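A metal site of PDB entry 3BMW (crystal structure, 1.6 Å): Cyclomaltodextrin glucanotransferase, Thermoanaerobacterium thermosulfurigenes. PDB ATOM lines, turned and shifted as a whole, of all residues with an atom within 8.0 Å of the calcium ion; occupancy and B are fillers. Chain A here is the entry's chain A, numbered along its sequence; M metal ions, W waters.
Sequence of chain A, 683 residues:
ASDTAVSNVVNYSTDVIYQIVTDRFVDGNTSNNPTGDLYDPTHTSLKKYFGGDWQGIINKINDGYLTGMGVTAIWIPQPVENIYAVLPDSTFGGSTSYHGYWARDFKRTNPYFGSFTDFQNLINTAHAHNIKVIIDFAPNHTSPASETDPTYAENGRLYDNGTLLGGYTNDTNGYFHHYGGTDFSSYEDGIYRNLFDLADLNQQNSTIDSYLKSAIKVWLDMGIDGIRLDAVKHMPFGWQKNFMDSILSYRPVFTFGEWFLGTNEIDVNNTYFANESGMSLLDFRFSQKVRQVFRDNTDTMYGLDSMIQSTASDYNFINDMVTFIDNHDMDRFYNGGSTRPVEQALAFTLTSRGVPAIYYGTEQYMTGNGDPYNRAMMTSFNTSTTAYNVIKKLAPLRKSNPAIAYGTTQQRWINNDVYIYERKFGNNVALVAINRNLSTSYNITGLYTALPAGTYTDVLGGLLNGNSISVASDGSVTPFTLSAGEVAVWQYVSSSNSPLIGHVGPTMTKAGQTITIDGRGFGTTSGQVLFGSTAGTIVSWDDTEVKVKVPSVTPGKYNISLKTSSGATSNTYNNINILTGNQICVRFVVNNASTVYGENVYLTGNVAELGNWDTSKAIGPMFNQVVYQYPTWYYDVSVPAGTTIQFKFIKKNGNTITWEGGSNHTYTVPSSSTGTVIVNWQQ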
ATOM      1  N   THR A  22      -4.641 -33.464  25.297  1.00  0.00           N
ATOM      2  CA  THR A  22      -3.868 -32.234  25.460  1.00  0.00           C
ATOM      3  C   THR A  22      -3.516 -31.566  24.129  1.00  0.00           C
ATOM      4  O   THR A  22      -3.763 -30.379  23.961  1.00  0.00           O
ATOM      5  CB  THR A  22      -2.592 -32.489  26.274  1.00  0.00           C
ATOM      6  OG1 THR A  22      -2.965 -32.915  27.592  1.00  0.00           O
ATOM      7  CG2 THR A  22      -1.748 -31.229  26.391  1.00  0.00           C
ATOM      8  N   ASP A  23      -2.958 -32.334  23.199  1.00  0.00           N
ATOM      9  CA  ASP A  23      -2.502 -31.775  21.928  1.00  0.00           C
ATOM     10  C   ASP A  23      -3.645 -31.156  21.115  1.00  0.00           C
ATOM     11  O   ASP A  23      -3.422 -30.300  20.259  1.00  0.00           O
ATOM     12  CB  ASP A  23      -1.813 -32.847  21.087  1.00  0.00           C
ATOM     13  CG  ASP A  23      -1.260 -32.288  19.793  1.00  0.00           C
ATOM     14  OD1 ASP A  23      -0.328 -31.455  19.857  1.00  0.00           O
ATOM     15  OD2 ASP A  23      -1.768 -32.656  18.711  1.00  0.00           O
ATOM     16  N   VAL A  26      -6.116 -26.823  23.553  1.00  0.00           N
ATOM     17  CA  VAL A  26      -5.742 -25.420  23.339  1.00  0.00           C
ATOM     18  C   VAL A  26      -4.216 -25.260  23.285  1.00  0.00           C
ATOM     19  O   VAL A  26      -3.505 -25.743  24.167  1.00  0.00           O
ATOM     20  CB  VAL A  26      -6.311 -24.495  24.457  1.00  0.00           C
ATOM     21  CG1 VAL A  26      -5.871 -23.045  24.243  1.00  0.00           C
ATOM     22  CG2 VAL A  26      -7.823 -24.584  24.498  1.00  0.00           C
ATOM     23  N   ASP A  27      -3.742 -24.611  22.229  1.00  0.00           N
ATOM     24  CA  ASP A  27      -2.329 -24.272  22.100  1.00  0.00           C
ATOM     25  C   ASP A  27      -2.068 -22.971  22.869  1.00  0.00           C
ATOM     26  O   ASP A  27      -2.210 -21.873  22.317  1.00  0.00           O
ATOM     27  CB  ASP A  27      -1.936 -24.143  20.613  1.00  0.00           C
ATOM     28  CG  ASP A  27      -0.471 -23.788  20.398  1.00  0.00           C
ATOM     29  OD1 ASP A  27       0.318 -23.802  21.377  1.00  0.00           O
ATOM     30  OD2 ASP A  27      -0.111 -23.473  19.236  1.00  0.00           O
ATOM     31  N   GLY A  28      -1.714 -23.097  24.143  1.00  0.00           N
ATOM     32  CA  GLY A  28      -1.519 -21.929  25.016  1.00  0.00           C
ATOM     33  C   GLY A  28      -0.140 -21.284  24.904  1.00  0.00           C
ATOM     34  O   GLY A  28       0.060 -20.152  25.354  1.00  0.00           O
ATOM     35  N   ASN A  29       0.816 -21.997  24.325  1.00  0.00           N
ATOM     36  CA  ASN A  29       2.140 -21.442  24.090  1.00  0.00           C
ATOM     37  C   ASN A  29       2.720 -21.959  22.786  1.00  0.00           C
ATOM     38  O   ASN A  29       3.009 -23.154  22.652  1.00  0.00           O
ATOM     39  CB  ASN A  29       3.091 -21.734  25.258  1.00  0.00           C
ATOM     40  CG  ASN A  29       4.438 -21.038  25.102  1.00  0.00           C
ATOM     41  OD1 ASN A  29       5.303 -21.529  24.393  1.00  0.00           O
ATOM     42  ND2 ASN A  29       4.609 -19.898  25.760  1.00  0.00           N
ATOM     43  N   THR A  30       2.886 -21.071  21.816  1.00  0.00           N
ATOM     44  CA  THR A  30       3.381 -21.486  20.500  1.00  0.00           C
ATOM     45  C   THR A  30       4.872 -21.828  20.514  1.00  0.00           C
ATOM     46  O   THR A  30       5.322 -22.624  19.689  1.00  0.00           O
ATOM     47  CB  THR A  30       3.084 -20.443  19.408  1.00  0.00           C
ATOM     48  OG1 THR A  30       3.680 -19.188  19.768  1.00  0.00           O
ATOM     49  CG2 THR A  30       1.584 -20.265  19.227  1.00  0.00           C
ATOM     50  N   SER A  31       5.629 -21.232  21.433  1.00  0.00           N
ATOM     51  CA  SER A  31       7.089 -21.433  21.468  1.00  0.00           C
ATOM     52  C   SER A  31       7.487 -22.867  21.792  1.00  0.00           C
ATOM     53  O   SER A  31       8.591 -23.292  21.456  1.00  0.00           O
ATOM     54  CB  SER A  31       7.783 -20.460  22.429  1.00  0.00           C
ATOM     55  OG  SER A  31       7.596 -20.859  23.777  1.00  0.00           O
ATOM     56  N   ASN A  32       6.589 -23.608  22.445  1.00  0.00           N
ATOM     57  CA  ASN A  32       6.852 -25.016  22.767  1.00  0.00           C
ATOM     58  C   ASN A  32       6.409 -26.009  21.679  1.00  0.00           C
ATOM     59  O   ASN A  32       6.600 -27.208  21.824  1.00  0.00           O
ATOM     60  CB  ASN A  32       6.285 -25.414  24.141  1.00  0.00           C
ATOM     61  CG  ASN A  32       4.760 -25.441  24.169  1.00  0.00           C
ATOM     62  OD1 ASN A  32       4.094 -25.598  23.157  1.00  0.00           O
ATOM     63  ND2 ASN A  32       4.205 -25.318  25.381  1.00  0.00           N
ATOM     64  N   ASN A  33       5.804 -25.497  20.617  1.00  0.00           N
ATOM     65  CA  ASN A  33       5.356 -26.341  19.507  1.00  0.00           C
ATOM     66  C   ASN A  33       6.526 -27.054  18.843  1.00  0.00           C
ATOM     67  O   ASN A  33       7.627 -26.491  18.742  1.00  0.00           O
ATOM     68  CB  ASN A  33       4.611 -25.516  18.448  1.00  0.00           C
ATOM     69  CG  ASN A  33       3.268 -25.013  18.925  1.00  0.00           C
ATOM     70  OD1 ASN A  33       2.748 -25.456  19.957  1.00  0.00           O
ATOM     71  ND2 ASN A  33       2.680 -24.087  18.176  1.00  0.00           N
ATOM     72  N   PRO A  34       6.308 -28.309  18.381  1.00  0.00           N
ATOM     73  CA  PRO A  34       7.337 -28.962  17.585  1.00  0.00           C
ATOM     74  C   PRO A  34       7.545 -28.197  16.280  1.00  0.00           C
ATOM     75  O   PRO A  34       6.696 -27.384  15.897  1.00  0.00           O
ATOM     76  CB  PRO A  34       6.747 -30.348  17.272  1.00  0.00           C
ATOM     77  CG  PRO A  34       5.580 -30.511  18.194  1.00  0.00           C
ATOM     78  CD  PRO A  34       5.106 -29.147  18.558  1.00  0.00           C
ATOM     79  N   TYR A  39       4.827 -31.264  13.281  1.00  0.00           N
ATOM     80  CA  TYR A  39       3.846 -30.218  13.591  1.00  0.00           C
ATOM     81  C   TYR A  39       2.989 -29.808  12.401  1.00  0.00           C
ATOM     82  O   TYR A  39       3.493 -29.589  11.298  1.00  0.00           O
ATOM     83  CB  TYR A  39       4.590 -28.992  14.158  1.00  0.00           C
ATOM     84  CG  TYR A  39       3.732 -27.780  14.463  1.00  0.00           C
ATOM     85  CD1 TYR A  39       2.657 -27.857  15.364  1.00  0.00           C
ATOM     86  CD2 TYR A  39       4.009 -26.551  13.885  1.00  0.00           C
ATOM     87  CE1 TYR A  39       1.875 -26.739  15.646  1.00  0.00           C
ATOM     88  CE2 TYR A  39       3.232 -25.428  14.156  1.00  0.00           C
ATOM     89  CZ  TYR A  39       2.163 -25.528  15.033  1.00  0.00           C
ATOM     90  OH  TYR A  39       1.396 -24.409  15.306  1.00  0.00           O
ATOM     91  N   TYR A  49       1.284 -33.441  15.671  1.00  0.00           N
ATOM     92  CA  TYR A  49       1.097 -32.502  16.779  1.00  0.00           C
ATOM     93  C   TYR A  49       0.409 -31.240  16.264  1.00  0.00           C
ATOM     94  O   TYR A  49       0.881 -30.623  15.293  1.00  0.00           O
ATOM     95  CB  TYR A  49       2.442 -32.122  17.407  1.00  0.00           C
ATOM     96  CG  TYR A  49       3.000 -33.100  18.438  1.00  0.00           C
ATOM     97  CD1 TYR A  49       3.716 -34.231  18.036  1.00  0.00           C
ATOM     98  CD2 TYR A  49       2.837 -32.873  19.801  1.00  0.00           C
ATOM     99  CE1 TYR A  49       4.236 -35.121  18.979  1.00  0.00           C
ATOM    100  CE2 TYR A  49       3.355 -33.760  20.753  1.00  0.00           C
ATOM    101  CZ  TYR A  49       4.051 -34.873  20.332  1.00  0.00           C
ATOM    102  OH  TYR A  49       4.576 -35.758  21.263  1.00  0.00           O
ATOM    103  N   PHE A  50      -0.695 -30.863  16.905  1.00  0.00           N
ATOM    104  CA  PHE A  50      -1.413 -29.631  16.588  1.00  0.00           C
ATOM    105  C   PHE A  50      -0.980 -28.481  17.514  1.00  0.00           C
ATOM    106  O   PHE A  50      -1.280 -27.320  17.243  1.00  0.00           O
ATOM    107  CB  PHE A  50      -2.917 -29.853  16.709  1.00  0.00           C
ATOM    108  CG  PHE A  50      -3.527 -30.635  15.551  1.00  0.00           C
ATOM    109  CD1 PHE A  50      -2.744 -31.144  14.520  1.00  0.00           C
ATOM    110  CD2 PHE A  50      -4.905 -30.884  15.534  1.00  0.00           C
ATOM    111  CE1 PHE A  50      -3.326 -31.874  13.473  1.00  0.00           C
ATOM    112  CE2 PHE A  50      -5.488 -31.610  14.497  1.00  0.00           C
ATOM    113  CZ  PHE A  50      -4.700 -32.111  13.463  1.00  0.00           C
ATOM    114  N   GLY A  51      -0.295 -28.827  18.610  1.00  0.00           N
ATOM    115  CA  GLY A  51       0.305 -27.826  19.498  1.00  0.00           C
ATOM    116  C   GLY A  51      -0.398 -27.568  20.818  1.00  0.00           C
ATOM    117  O   GLY A  51       0.049 -26.714  21.604  1.00  0.00           O
ATOM    118  N   GLY A  52      -1.488 -28.287  21.081  1.00  0.00           N
ATOM    119  CA  GLY A  52      -2.200 -28.140  22.365  1.00  0.00           C
ATOM    120  C   GLY A  52      -1.309 -28.519  23.525  1.00  0.00           C
ATOM    121  O   GLY A  52      -0.531 -29.481  23.443  1.00  0.00           O
ATOM    122  N   ASP A  53      -1.406 -27.785  24.619  1.00  0.00           N
ATOM    123  CA  ASP A  53      -0.435 -27.938  25.697  1.00  0.00           C
ATOM    124  C   ASP A  53      -1.041 -27.657  27.072  1.00  0.00           C
ATOM    125  O   ASP A  53      -2.225 -27.334  27.191  1.00  0.00           O
ATOM    126  CB  ASP A  53       0.797 -27.063  25.425  1.00  0.00           C
ATOM    127  CG  ASP A  53       0.446 -25.610  25.131  1.00  0.00           C
ATOM    128  OD1 ASP A  53      -0.506 -25.109  25.754  1.00  0.00           O
ATOM    129  OD2 ASP A  53       1.097 -24.991  24.252  1.00  0.00           O
ATOM    130  N   TRP A  54      -0.207 -27.781  28.115  1.00  0.00           N
ATOM    131  CA  TRP A  54      -0.697 -27.599  29.483  1.00  0.00           C
ATOM    132  C   TRP A  54      -1.087 -26.158  29.786  1.00  0.00           C
ATOM    133  O   TRP A  54      -2.053 -25.921  30.522  1.00  0.00           O
ATOM    134  CB  TRP A  54       0.316 -28.132  30.508  1.00  0.00           C
ATOM    135  CG  TRP A  54       0.541 -29.629  30.389  1.00  0.00           C
ATOM    136  CD1 TRP A  54      -0.378 -30.584  30.018  1.00  0.00           C
ATOM    137  CD2 TRP A  54       1.759 -30.346  30.658  1.00  0.00           C
ATOM    138  NE1 TRP A  54       0.199 -31.833  30.028  1.00  0.00           N
ATOM    139  CE2 TRP A  54       1.507 -31.714  30.425  1.00  0.00           C
ATOM    140  CE3 TRP A  54       3.043 -29.950  31.072  1.00  0.00           C
ATOM    141  CZ2 TRP A  54       2.498 -32.697  30.574  1.00  0.00           C
ATOM    142  CZ3 TRP A  54       4.020 -30.935  31.231  1.00  0.00           C
ATOM    143  CH2 TRP A  54       3.742 -32.294  30.981  1.00  0.00           C
ATOM    144  N   GLN A  55      -0.369 -25.205  29.201  1.00  0.00           N
ATOM    145  CA  GLN A  55      -0.745 -23.793  29.313  1.00  0.00           C
ATOM    146  C   GLN A  55      -2.158 -23.559  28.769  1.00  0.00           C
ATOM    147  O   GLN A  55      -2.938 -22.812  29.344  1.00  0.00           O
ATOM    148  CB  GLN A  55       0.258 -22.877  28.609  1.00  0.00           C
ATOM    149  CG  GLN A  55      -0.066 -21.396  28.734  1.00  0.00           C
ATOM    150  CD  GLN A  55      -0.066 -20.913  30.183  1.00  0.00           C
ATOM    151  OE1 GLN A  55       0.864 -21.185  30.947  1.00  0.00           O
ATOM    152  NE2 GLN A  55      -1.110 -20.190  30.557  1.00  0.00           N
ATOM    153  N   GLY A  56      -2.477 -24.206  27.646  1.00  0.00           N
ATOM    154  CA  GLY A  56      -3.823 -24.132  27.080  1.00  0.00           C
ATOM    155  C   GLY A  56      -4.903 -24.600  28.044  1.00  0.00           C
ATOM    156  O   GLY A  56      -5.974 -23.966  28.150  1.00  0.00           O
ATOM    157  N   PRO A 111       8.170 -32.264  26.201  1.00  0.00           N
ATOM    158  CA  PRO A 111       8.412 -30.811  26.190  1.00  0.00           C
ATOM    159  C   PRO A 111       7.394 -30.053  25.362  1.00  0.00           C
ATOM    160  O   PRO A 111       7.253 -28.830  25.501  1.00  0.00           O
ATOM    161  CB  PRO A 111       9.813 -30.689  25.551  1.00  0.00           C
ATOM    162  CG  PRO A 111       9.989 -31.941  24.755  1.00  0.00           C
ATOM    163  CD  PRO A 111       9.255 -33.013  25.541  1.00  0.00           C
ATOM    164  N   TYR A 112       6.660 -30.760  24.506  1.00  0.00           N
ATOM    165  CA  TYR A 112       5.653 -30.124  23.679  1.00  0.00           C
ATOM    166  C   TYR A 112       4.411 -29.773  24.497  1.00  0.00           C
ATOM    167  O   TYR A 112       3.724 -28.793  24.220  1.00  0.00           O
ATOM    168  CB  TYR A 112       5.309 -30.995  22.472  1.00  0.00           C
ATOM    169  CG  TYR A 112       6.527 -31.323  21.612  1.00  0.00           C
ATOM    170  CD1 TYR A 112       7.419 -30.327  21.210  1.00  0.00           C
ATOM    171  CD2 TYR A 112       6.768 -32.639  21.186  1.00  0.00           C
ATOM    172  CE1 TYR A 112       8.540 -30.626  20.426  1.00  0.00           C
ATOM    173  CE2 TYR A 112       7.885 -32.950  20.396  1.00  0.00           C
ATOM    174  CZ  TYR A 112       8.758 -31.936  20.017  1.00  0.00           C
ATOM    175  OH  TYR A 112       9.847 -32.253  19.236  1.00  0.00           O
ATOM    176  N   PHE A 113       4.131 -30.583  25.523  1.00  0.00           N
ATOM    177  CA  PHE A 113       3.058 -30.262  26.464  1.00  0.00           C
ATOM    178  C   PHE A 113       3.543 -29.221  27.475  1.00  0.00           C
ATOM    179  O   PHE A 113       2.784 -28.343  27.898  1.00  0.00           O
ATOM    180  CB  PHE A 113       2.573 -31.505  27.207  1.00  0.00           C
ATOM    181  CG  PHE A 113       1.946 -32.584  26.323  1.00  0.00           C
ATOM    182  CD1 PHE A 113       1.507 -32.315  25.022  1.00  0.00           C
ATOM    183  CD2 PHE A 113       1.785 -33.870  26.837  1.00  0.00           C
ATOM    184  CE1 PHE A 113       0.928 -33.331  24.238  1.00  0.00           C
ATOM    185  CE2 PHE A 113       1.201 -34.892  26.065  1.00  0.00           C
ATOM    186  CZ  PHE A 113       0.774 -34.618  24.764  1.00  0.00           C
ATOM    187  N   GLY A 114       4.812 -29.319  27.860  1.00  0.00           N
ATOM    188  CA  GLY A 114       5.410 -28.354  28.782  1.00  0.00           C
ATOM    189  C   GLY A 114       6.549 -28.918  29.617  1.00  0.00           C
ATOM    190  O   GLY A 114       6.898 -30.089  29.513  1.00  0.00           O
HETATM  191 CA    CA M   1       2.006 -25.396  22.152  1.00  0.00          CA
HETATM  192  O   HOH W   1       2.744 -27.728  21.976  1.00  0.00           O
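The side-chain hydroxyl (OG) of Ser 31 lies within hydrogen-bond range of the side-chain amide oxygen (OD1) of Asn 29 (2.5 Å).
ND2 of Asn 33 sits close to O of Thr 30 (3.4 Å).
N of Asp 53 is in hydrogen-bond range of O of Val 26 (3.0 Å).
O of Tyr 112 lies close to OD1 of Asn 32 (3.4 Å).
The backbone NH of Gly 51 is in hydrogen-bond range of the side-chain carboxylate of Asp 23, at 2.9 Å.
The backbone NH of Gly 56 sits at hydrogen-bond distance from the side-chain carboxylate of Asp 53 (2.9 Å).
The side-chain carboxylate (OD1) of Asp 53 lies within hydrogen-bond range of the backbone NH (N) of Gly 28 (2.8 Å).
The side-chain carboxylate of Asp 53 sits close to the backbone NH of Gln 55, 3.5 Å away.
Within 4 Å of the calcium ion: Asp 27, Asn 29, Asn 32, Asn 33, Gly 51 and Asp 53.
The nearest printed residue that does not touch the calcium ion is Tyr 112 (4.3 Å).
The calcium ion is bound by the side-chain amide oxygen of Asn 33 (2.3 Å), the side-chain carboxylate of Asp 53 (2.3 Å), the side-chain amide oxygen of Asn 32 (2.3 Å), the backbone carbonyl oxygen of Gly 51 (2.4 Å), the side-chain carboxylate of Asp 27 (2.4 Å), water W1 (2.5 Å) and the backbone carbonyl oxygen of Asn 29 (2.5 Å).
The calcium ion has seven donor atoms within binding distance.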
